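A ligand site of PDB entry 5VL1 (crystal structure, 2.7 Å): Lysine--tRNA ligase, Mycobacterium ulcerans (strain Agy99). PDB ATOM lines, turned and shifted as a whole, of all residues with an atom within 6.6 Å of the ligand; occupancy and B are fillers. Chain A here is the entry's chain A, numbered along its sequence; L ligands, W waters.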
ATOM      1  N   GLY A 217     -26.129  33.908  17.564  1.00  0.00           N
ATOM      2  CA  GLY A 217     -25.801  32.531  17.280  1.00  0.00           C
ATOM      3  C   GLY A 217     -26.660  31.510  17.995  1.00  0.00           C
ATOM      4  O   GLY A 217     -26.513  30.310  17.724  1.00  0.00           O
ATOM      5  N   ALA A 218     -27.534  31.936  18.897  1.00  0.00           N
ATOM      6  CA  ALA A 218     -28.399  31.036  19.637  1.00  0.00           C
ATOM      7  C   ALA A 218     -29.529  31.849  20.260  1.00  0.00           C
ATOM      8  O   ALA A 218     -29.518  33.081  20.239  1.00  0.00           O
ATOM      9  CB  ALA A 218     -27.632  30.254  20.705  1.00  0.00           C
ATOM     10  N   ALA A 219     -30.503  31.140  20.804  1.00  0.00           N
ATOM     11  CA  ALA A 219     -31.643  31.753  21.505  1.00  0.00           C
ATOM     12  C   ALA A 219     -31.430  31.571  23.006  1.00  0.00           C
ATOM     13  O   ALA A 219     -31.842  30.571  23.597  1.00  0.00           O
ATOM     14  CB  ALA A 219     -32.951  31.141  21.038  1.00  0.00           C
ATOM     15  N   ILE A 238     -22.880  33.571  23.649  1.00  0.00           N
ATOM     16  CA  ILE A 238     -23.781  32.445  23.832  1.00  0.00           C
ATOM     17  C   ILE A 238     -23.533  31.350  22.810  1.00  0.00           C
ATOM     18  O   ILE A 238     -23.991  30.223  22.998  1.00  0.00           O
ATOM     19  CB  ILE A 238     -25.249  32.911  23.784  1.00  0.00           C
ATOM     20  CG1 ILE A 238     -25.551  33.573  22.445  1.00  0.00           C
ATOM     21  CG2 ILE A 238     -25.537  33.872  24.924  1.00  0.00           C
ATOM     22  CD1 ILE A 238     -26.954  34.103  22.353  1.00  0.00           C
ATOM     23  N   ALA A 239     -22.800  31.655  21.736  1.00  0.00           N
ATOM     24  CA  ALA A 239     -22.452  30.716  20.689  1.00  0.00           C
ATOM     25  C   ALA A 239     -21.370  31.336  19.806  1.00  0.00           C
ATOM     26  O   ALA A 239     -21.365  32.555  19.603  1.00  0.00           O
ATOM     27  CB  ALA A 239     -23.677  30.363  19.844  1.00  0.00           C
ATOM     28  N   PRO A 240     -20.456  30.535  19.263  1.00  0.00           N
ATOM     29  CA  PRO A 240     -19.496  31.051  18.278  1.00  0.00           C
ATOM     30  C   PRO A 240     -19.988  31.031  16.840  1.00  0.00           C
ATOM     31  O   PRO A 240     -19.190  31.278  15.934  1.00  0.00           O
ATOM     32  CB  PRO A 240     -18.317  30.084  18.450  1.00  0.00           C
ATOM     33  CG  PRO A 240     -18.980  28.784  18.775  1.00  0.00           C
ATOM     34  CD  PRO A 240     -20.187  29.137  19.616  1.00  0.00           C
ATOM     35  N   GLU A 241     -21.281  30.747  16.622  1.00  0.00           N
ATOM     36  CA  GLU A 241     -21.784  30.470  15.277  1.00  0.00           C
ATOM     37  C   GLU A 241     -21.542  31.640  14.322  1.00  0.00           C
ATOM     38  O   GLU A 241     -21.027  31.444  13.212  1.00  0.00           O
ATOM     39  CB  GLU A 241     -23.284  30.142  15.340  1.00  0.00           C
ATOM     40  CG  GLU A 241     -23.986  30.158  13.985  1.00  0.00           C
ATOM     41  CD  GLU A 241     -25.212  29.261  13.948  1.00  0.00           C
ATOM     42  OE1 GLU A 241     -25.627  28.773  15.022  1.00  0.00           O
ATOM     43  OE2 GLU A 241     -25.752  29.042  12.845  1.00  0.00           O
ATOM     44  N   LYS A 245     -19.005  31.419  11.039  1.00  0.00           N
ATOM     45  CA  LYS A 245     -19.468  31.638   9.670  1.00  0.00           C
ATOM     46  C   LYS A 245     -18.664  32.717   8.973  1.00  0.00           C
ATOM     47  O   LYS A 245     -18.440  32.632   7.759  1.00  0.00           O
ATOM     48  CB  LYS A 245     -20.957  31.998   9.668  1.00  0.00           C
ATOM     49  CG  LYS A 245     -21.852  30.833  10.037  1.00  0.00           C
ATOM     50  CD  LYS A 245     -23.312  31.183   9.827  1.00  0.00           C
ATOM     51  CE  LYS A 245     -24.201  30.028  10.246  1.00  0.00           C
ATOM     52  NZ  LYS A 245     -25.629  30.230   9.865  1.00  0.00           N
ATOM     53  N   ARG A 263     -24.448  31.148  29.031  1.00  0.00           N
ATOM     54  CA  ARG A 263     -25.868  31.394  28.845  1.00  0.00           C
ATOM     55  C   ARG A 263     -26.499  31.640  30.208  1.00  0.00           C
ATOM     56  O   ARG A 263     -26.383  30.808  31.112  1.00  0.00           O
ATOM     57  CB  ARG A 263     -26.552  30.230  28.125  1.00  0.00           C
ATOM     58  CG  ARG A 263     -26.019  30.050  26.717  1.00  0.00           C
ATOM     59  CD  ARG A 263     -26.679  28.928  25.955  1.00  0.00           C
ATOM     60  NE  ARG A 263     -26.023  28.766  24.659  1.00  0.00           N
ATOM     61  CZ  ARG A 263     -26.406  27.905  23.721  1.00  0.00           C
ATOM     62  NH1 ARG A 263     -27.452  27.119  23.926  1.00  0.00           N
ATOM     63  NH2 ARG A 263     -25.728  27.834  22.580  1.00  0.00           N
ATOM     64  N   MET A 277     -18.593  23.814  24.545  1.00  0.00           N
ATOM     65  CA  MET A 277     -19.375  23.549  23.350  1.00  0.00           C
ATOM     66  C   MET A 277     -18.474  23.301  22.147  1.00  0.00           C
ATOM     67  O   MET A 277     -17.431  23.950  22.001  1.00  0.00           O
ATOM     68  CB  MET A 277     -20.312  24.723  23.029  1.00  0.00           C
ATOM     69  CG  MET A 277     -21.120  24.522  21.772  1.00  0.00           C
ATOM     70  SD  MET A 277     -22.858  24.192  22.060  1.00  0.00           S
ATOM     71  CE  MET A 277     -23.543  25.703  21.398  1.00  0.00           C
ATOM     72  N   LEU A 278     -18.876  22.358  21.304  1.00  0.00           N
ATOM     73  CA  LEU A 278     -18.237  22.100  20.029  1.00  0.00           C
ATOM     74  C   LEU A 278     -19.131  22.610  18.906  1.00  0.00           C
ATOM     75  O   LEU A 278     -20.303  22.231  18.832  1.00  0.00           O
ATOM     76  CB  LEU A 278     -17.954  20.606  19.838  1.00  0.00           C
ATOM     77  CG  LEU A 278     -17.554  20.184  18.424  1.00  0.00           C
ATOM     78  CD1 LEU A 278     -16.189  20.740  18.077  1.00  0.00           C
ATOM     79  CD2 LEU A 278     -17.581  18.670  18.281  1.00  0.00           C
ATOM     80  N   GLU A 279     -18.588  23.449  18.042  1.00  0.00           N
ATOM     81  CA  GLU A 279     -19.252  23.840  16.805  1.00  0.00           C
ATOM     82  C   GLU A 279     -18.305  23.594  15.639  1.00  0.00           C
ATOM     83  O   GLU A 279     -17.139  23.984  15.701  1.00  0.00           O
ATOM     84  CB  GLU A 279     -19.707  25.302  16.817  1.00  0.00           C
ATOM     85  CG  GLU A 279     -20.982  25.563  17.598  1.00  0.00           C
ATOM     86  CD  GLU A 279     -21.659  26.855  17.178  1.00  0.00           C
ATOM     87  OE1 GLU A 279     -21.368  27.355  16.071  1.00  0.00           O
ATOM     88  OE2 GLU A 279     -22.488  27.373  17.960  1.00  0.00           O
ATOM     89  N   THR A 280     -18.801  22.926  14.605  1.00  0.00           N
ATOM     90  CA  THR A 280     -18.027  22.645  13.405  1.00  0.00           C
ATOM     91  C   THR A 280     -18.744  23.211  12.187  1.00  0.00           C
ATOM     92  O   THR A 280     -19.969  23.276  12.149  1.00  0.00           O
ATOM     93  CB  THR A 280     -17.815  21.126  13.204  1.00  0.00           C
ATOM     94  OG1 THR A 280     -19.048  20.533  12.791  1.00  0.00           O
ATOM     95  CG2 THR A 280     -17.340  20.471  14.497  1.00  0.00           C
ATOM     96  N   TYR A 281     -17.954  23.655  11.199  1.00  0.00           N
ATOM     97  CA  TYR A 281     -18.514  24.153   9.948  1.00  0.00           C
ATOM     98  C   TYR A 281     -17.693  23.603   8.790  1.00  0.00           C
ATOM     99  O   TYR A 281     -16.463  23.613   8.828  1.00  0.00           O
ATOM    100  CB  TYR A 281     -18.566  25.687   9.928  1.00  0.00           C
ATOM    101  CG  TYR A 281     -19.615  26.204  10.885  1.00  0.00           C
ATOM    102  CD1 TYR A 281     -19.308  26.389  12.231  1.00  0.00           C
ATOM    103  CD2 TYR A 281     -20.907  26.463  10.458  1.00  0.00           C
ATOM    104  CE1 TYR A 281     -20.275  26.830  13.120  1.00  0.00           C
ATOM    105  CE2 TYR A 281     -21.874  26.904  11.347  1.00  0.00           C
ATOM    106  CZ  TYR A 281     -21.549  27.082  12.677  1.00  0.00           C
ATOM    107  OH  TYR A 281     -22.492  27.521  13.569  1.00  0.00           O
ATOM    108  N   LEU A 401     -31.410  30.672  11.522  1.00  0.00           N
ATOM    109  CA  LEU A 401     -30.119  30.589  10.854  1.00  0.00           C
ATOM    110  C   LEU A 401     -30.011  29.362   9.954  1.00  0.00           C
ATOM    111  O   LEU A 401     -28.929  29.080   9.441  1.00  0.00           O
ATOM    112  CB  LEU A 401     -28.985  30.590  11.882  1.00  0.00           C
ATOM    113  CG  LEU A 401     -28.947  31.774  12.859  1.00  0.00           C
ATOM    114  CD1 LEU A 401     -27.883  31.555  13.928  1.00  0.00           C
ATOM    115  CD2 LEU A 401     -28.705  33.088  12.131  1.00  0.00           C
ATOM    116  N   THR A 402     -31.099  28.640   9.750  1.00  0.00           N
ATOM    117  CA  THR A 402     -31.099  27.401   8.994  1.00  0.00           C
ATOM    118  C   THR A 402     -31.709  27.631   7.613  1.00  0.00           C
ATOM    119  O   THR A 402     -32.731  28.324   7.485  1.00  0.00           O
ATOM    120  CB  THR A 402     -31.864  26.311   9.745  1.00  0.00           C
ATOM    121  OG1 THR A 402     -31.435  26.283  11.111  1.00  0.00           O
ATOM    122  CG2 THR A 402     -31.611  24.957   9.109  1.00  0.00           C
ATOM    123  N   GLU A 423     -31.403  15.496  24.156  1.00  0.00           N
ATOM    124  CA  GLU A 423     -30.941  16.251  23.003  1.00  0.00           C
ATOM    125  C   GLU A 423     -29.434  16.463  23.101  1.00  0.00           C
ATOM    126  O   GLU A 423     -28.955  17.116  24.035  1.00  0.00           O
ATOM    127  CB  GLU A 423     -31.676  17.584  22.915  1.00  0.00           C
ATOM    128  CG  GLU A 423     -31.202  18.523  21.831  1.00  0.00           C
ATOM    129  CD  GLU A 423     -32.018  19.808  21.776  1.00  0.00           C
ATOM    130  OE1 GLU A 423     -31.522  20.800  21.200  1.00  0.00           O
ATOM    131  OE2 GLU A 423     -33.140  19.826  22.330  1.00  0.00           O
ATOM    132  N   THR A 426     -26.906  19.020  17.177  1.00  0.00           N
ATOM    133  CA  THR A 426     -27.762  19.634  16.177  1.00  0.00           C
ATOM    134  C   THR A 426     -26.929  19.991  14.952  1.00  0.00           C
ATOM    135  O   THR A 426     -25.734  20.288  15.071  1.00  0.00           O
ATOM    136  CB  THR A 426     -28.476  20.883  16.733  1.00  0.00           C
ATOM    137  OG1 THR A 426     -29.417  21.374  15.765  1.00  0.00           O
ATOM    138  CG2 THR A 426     -27.472  21.984  17.057  1.00  0.00           C
ATOM    139  N   GLY A 427     -27.561  19.938  13.775  1.00  0.00           N
ATOM    140  CA  GLY A 427     -26.865  20.281  12.552  1.00  0.00           C
ATOM    141  C   GLY A 427     -27.749  20.996  11.536  1.00  0.00           C
ATOM    142  O   GLY A 427     -28.915  20.663  11.381  1.00  0.00           O
ATOM    143  N   TYR A 428     -27.185  21.988  10.844  1.00  0.00           N
ATOM    144  CA  TYR A 428     -27.933  22.771   9.879  1.00  0.00           C
ATOM    145  C   TYR A 428     -27.337  22.621   8.482  1.00  0.00           C
ATOM    146  O   TYR A 428     -26.147  22.359   8.320  1.00  0.00           O
ATOM    147  CB  TYR A 428     -27.947  24.282  10.215  1.00  0.00           C
ATOM    148  CG  TYR A 428     -28.470  24.705  11.578  1.00  0.00           C
ATOM    149  CD1 TYR A 428     -29.114  23.804  12.420  1.00  0.00           C
ATOM    150  CD2 TYR A 428     -28.320  26.006  12.016  1.00  0.00           C
ATOM    151  CE1 TYR A 428     -29.584  24.194  13.660  1.00  0.00           C
ATOM    152  CE2 TYR A 428     -28.780  26.411  13.248  1.00  0.00           C
ATOM    153  CZ  TYR A 428     -29.406  25.504  14.074  1.00  0.00           C
ATOM    154  OH  TYR A 428     -29.874  25.915  15.308  1.00  0.00           O
ATOM    155  N   GLU A 430     -26.577  25.485   6.348  1.00  0.00           N
ATOM    156  CA  GLU A 430     -26.480  26.873   6.761  1.00  0.00           C
ATOM    157  C   GLU A 430     -27.157  27.805   5.773  1.00  0.00           C
ATOM    158  O   GLU A 430     -27.084  27.622   4.555  1.00  0.00           O
ATOM    159  CB  GLU A 430     -25.023  27.281   6.948  1.00  0.00           C
ATOM    160  CG  GLU A 430     -24.286  26.504   8.038  1.00  0.00           C
ATOM    161  CD  GLU A 430     -25.029  26.488   9.381  1.00  0.00           C
ATOM    162  OE1 GLU A 430     -24.898  25.487  10.102  1.00  0.00           O
ATOM    163  OE2 GLU A 430     -25.740  27.462   9.710  1.00  0.00           O
ATOM    164  N   THR A 474     -22.384  23.282   6.026  1.00  0.00           N
ATOM    165  CA  THR A 474     -23.197  22.661   7.070  1.00  0.00           C
ATOM    166  C   THR A 474     -22.479  22.826   8.394  1.00  0.00           C
ATOM    167  O   THR A 474     -21.253  22.668   8.478  1.00  0.00           O
ATOM    168  CB  THR A 474     -23.471  21.177   6.773  1.00  0.00           C
ATOM    169  OG1 THR A 474     -24.194  20.597   7.859  1.00  0.00           O
ATOM    170  CG2 THR A 474     -22.172  20.400   6.561  1.00  0.00           C
ATOM    171  N   GLY A 475     -23.244  23.161   9.432  1.00  0.00           N
ATOM    172  CA  GLY A 475     -22.680  23.393  10.742  1.00  0.00           C
ATOM    173  C   GLY A 475     -23.338  22.536  11.800  1.00  0.00           C
ATOM    174  O   GLY A 475     -24.531  22.244  11.744  1.00  0.00           O
ATOM    175  N   THR A 476     -22.527  22.121  12.776  1.00  0.00           N
ATOM    176  CA  THR A 476     -23.002  21.295  13.875  1.00  0.00           C
ATOM    177  C   THR A 476     -22.752  21.980  15.210  1.00  0.00           C
ATOM    178  O   THR A 476     -21.894  22.872  15.326  1.00  0.00           O
ATOM    179  CB  THR A 476     -22.327  19.916  13.899  1.00  0.00           C
ATOM    180  OG1 THR A 476     -20.956  20.072  14.296  1.00  0.00           O
ATOM    181  CG2 THR A 476     -22.384  19.260  12.536  1.00  0.00           C
ATOM    182  N   GLY A 477     -23.490  21.535  16.211  1.00  0.00           N
ATOM    183  CA  GLY A 477     -23.291  21.958  17.580  1.00  0.00           C
ATOM    184  C   GLY A 477     -23.515  20.809  18.546  1.00  0.00           C
ATOM    185  O   GLY A 477     -24.426  20.001  18.351  1.00  0.00           O
ATOM    186  N   MET A 478     -22.678  20.703  19.574  1.00  0.00           N
ATOM    187  CA  MET A 478     -22.807  19.616  20.530  1.00  0.00           C
ATOM    188  C   MET A 478     -22.094  20.001  21.819  1.00  0.00           C
ATOM    189  O   MET A 478     -20.910  20.355  21.784  1.00  0.00           O
ATOM    190  CB  MET A 478     -22.223  18.315  19.961  1.00  0.00           C
ATOM    191  CG  MET A 478     -22.321  17.121  20.900  1.00  0.00           C
ATOM    192  SD  MET A 478     -21.682  15.602  20.157  1.00  0.00           S
ATOM    193  CE  MET A 478     -19.996  16.076  19.829  1.00  0.00           C
HETATM  194  N1  LIG L   1     -25.223  27.711  17.477  1.00  0.00           N
HETATM  195  C1  LIG L   1     -25.931  26.448  17.688  1.00  0.00           C
HETATM  196  C2  LIG L   1     -26.422  26.340  19.123  1.00  0.00           C
HETATM  197  O1  LIG L   1     -27.265  25.504  19.462  1.00  0.00           O
HETATM  198  C3  LIG L   1     -25.020  25.271  17.346  1.00  0.00           C
HETATM  199  C4  LIG L   1     -25.282  24.666  15.972  1.00  0.00           C
HETATM  200  C5  LIG L   1     -25.000  25.656  14.872  1.00  0.00           C
HETATM  201  C6  LIG L   1     -25.294  25.074  13.504  1.00  0.00           C
HETATM  202  N2  LIG L   1     -25.042  26.085  12.432  1.00  0.00           N
HETATM  203  O2  LIG L   1     -25.994  27.109  19.991  1.00  0.00           O
HETATM  204  O   HOH W   1     -29.936  24.213  17.649  1.00  0.00           O
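A nitrogen (N2) of the ligand lies within salt-bridge range of the side-chain carboxylate of Glu 430, at 2.4 Å. The side-chain hydroxyl (OH) of Tyr 281 sits at hydrogen-bond distance from a nitrogen (N2) of the ligand. The backbone carbonyl oxygen of Gly 217 lies within hydrogen-bond range of a nitrogen (N1) of the ligand (2.9 Å). An oxygen (O2) of the ligand lies within salt-bridge range of the guanidinium group (NH2) of Arg 263 (2.7 Å). N1 of the ligand is in salt-bridge range of OE1 of Glu 241 (2.7 Å). The side-chain carboxylate (OE2) of Glu 279 is in salt-bridge range of a nitrogen (N1) of the ligand (2.8 Å).
The side-chain hydroxyl of Tyr 281 sits at hydrogen-bond distance from the side-chain carboxylate of Glu 279, 2.7 Å away. OE1 of Glu 279 sits close to N of Glu 241 (3.4 Å). The side-chain carboxylate (OE1) of Glu 430 is in hydrogen-bond range of the backbone NH (N) of Gly 475 (2.9 Å). The backbone NH (N) of Gly 477 is in hydrogen-bond range of the backbone carbonyl oxygen (O) of Thr 426 (2.8 Å). The backbone NH (N) of Tyr 428 sits at hydrogen-bond distance from the backbone carbonyl oxygen (O) of Gly 475. The side-chain hydroxyl of Thr 476 sits at hydrogen-bond distance from the side-chain hydroxyl of Thr 280, 2.5 Å away. The side-chain amino group (NZ) of Lys 245 is in salt-bridge range of the side-chain carboxylate (OE2) of Glu 241. The backbone carbonyl oxygen of Ile 238 lies within hydrogen-bond range of the guanidinium group of Arg 263, at 3.0 Å.
Residues that only touch the ligand: Ala 218, Ala 239, Met 277, Thr 426, Tyr 428, Gly 475, Thr 476 and Gly 477. Hydrophobic or aromatic side chains within 4 Å of the ligand: Ala 218, Ala 239, Met 277, Tyr 281 and Tyr 428. The nearest printed residue that does not touch the ligand is Lys 245 (4.6 Å).
Water W1 lies within hydrogen-bond range of the side-chain hydroxyl of Tyr 428 (2.9 Å), the side-chain hydroxyl of Thr 426 (3.4 Å) and an oxygen (O1) of the ligand (3.5 Å).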
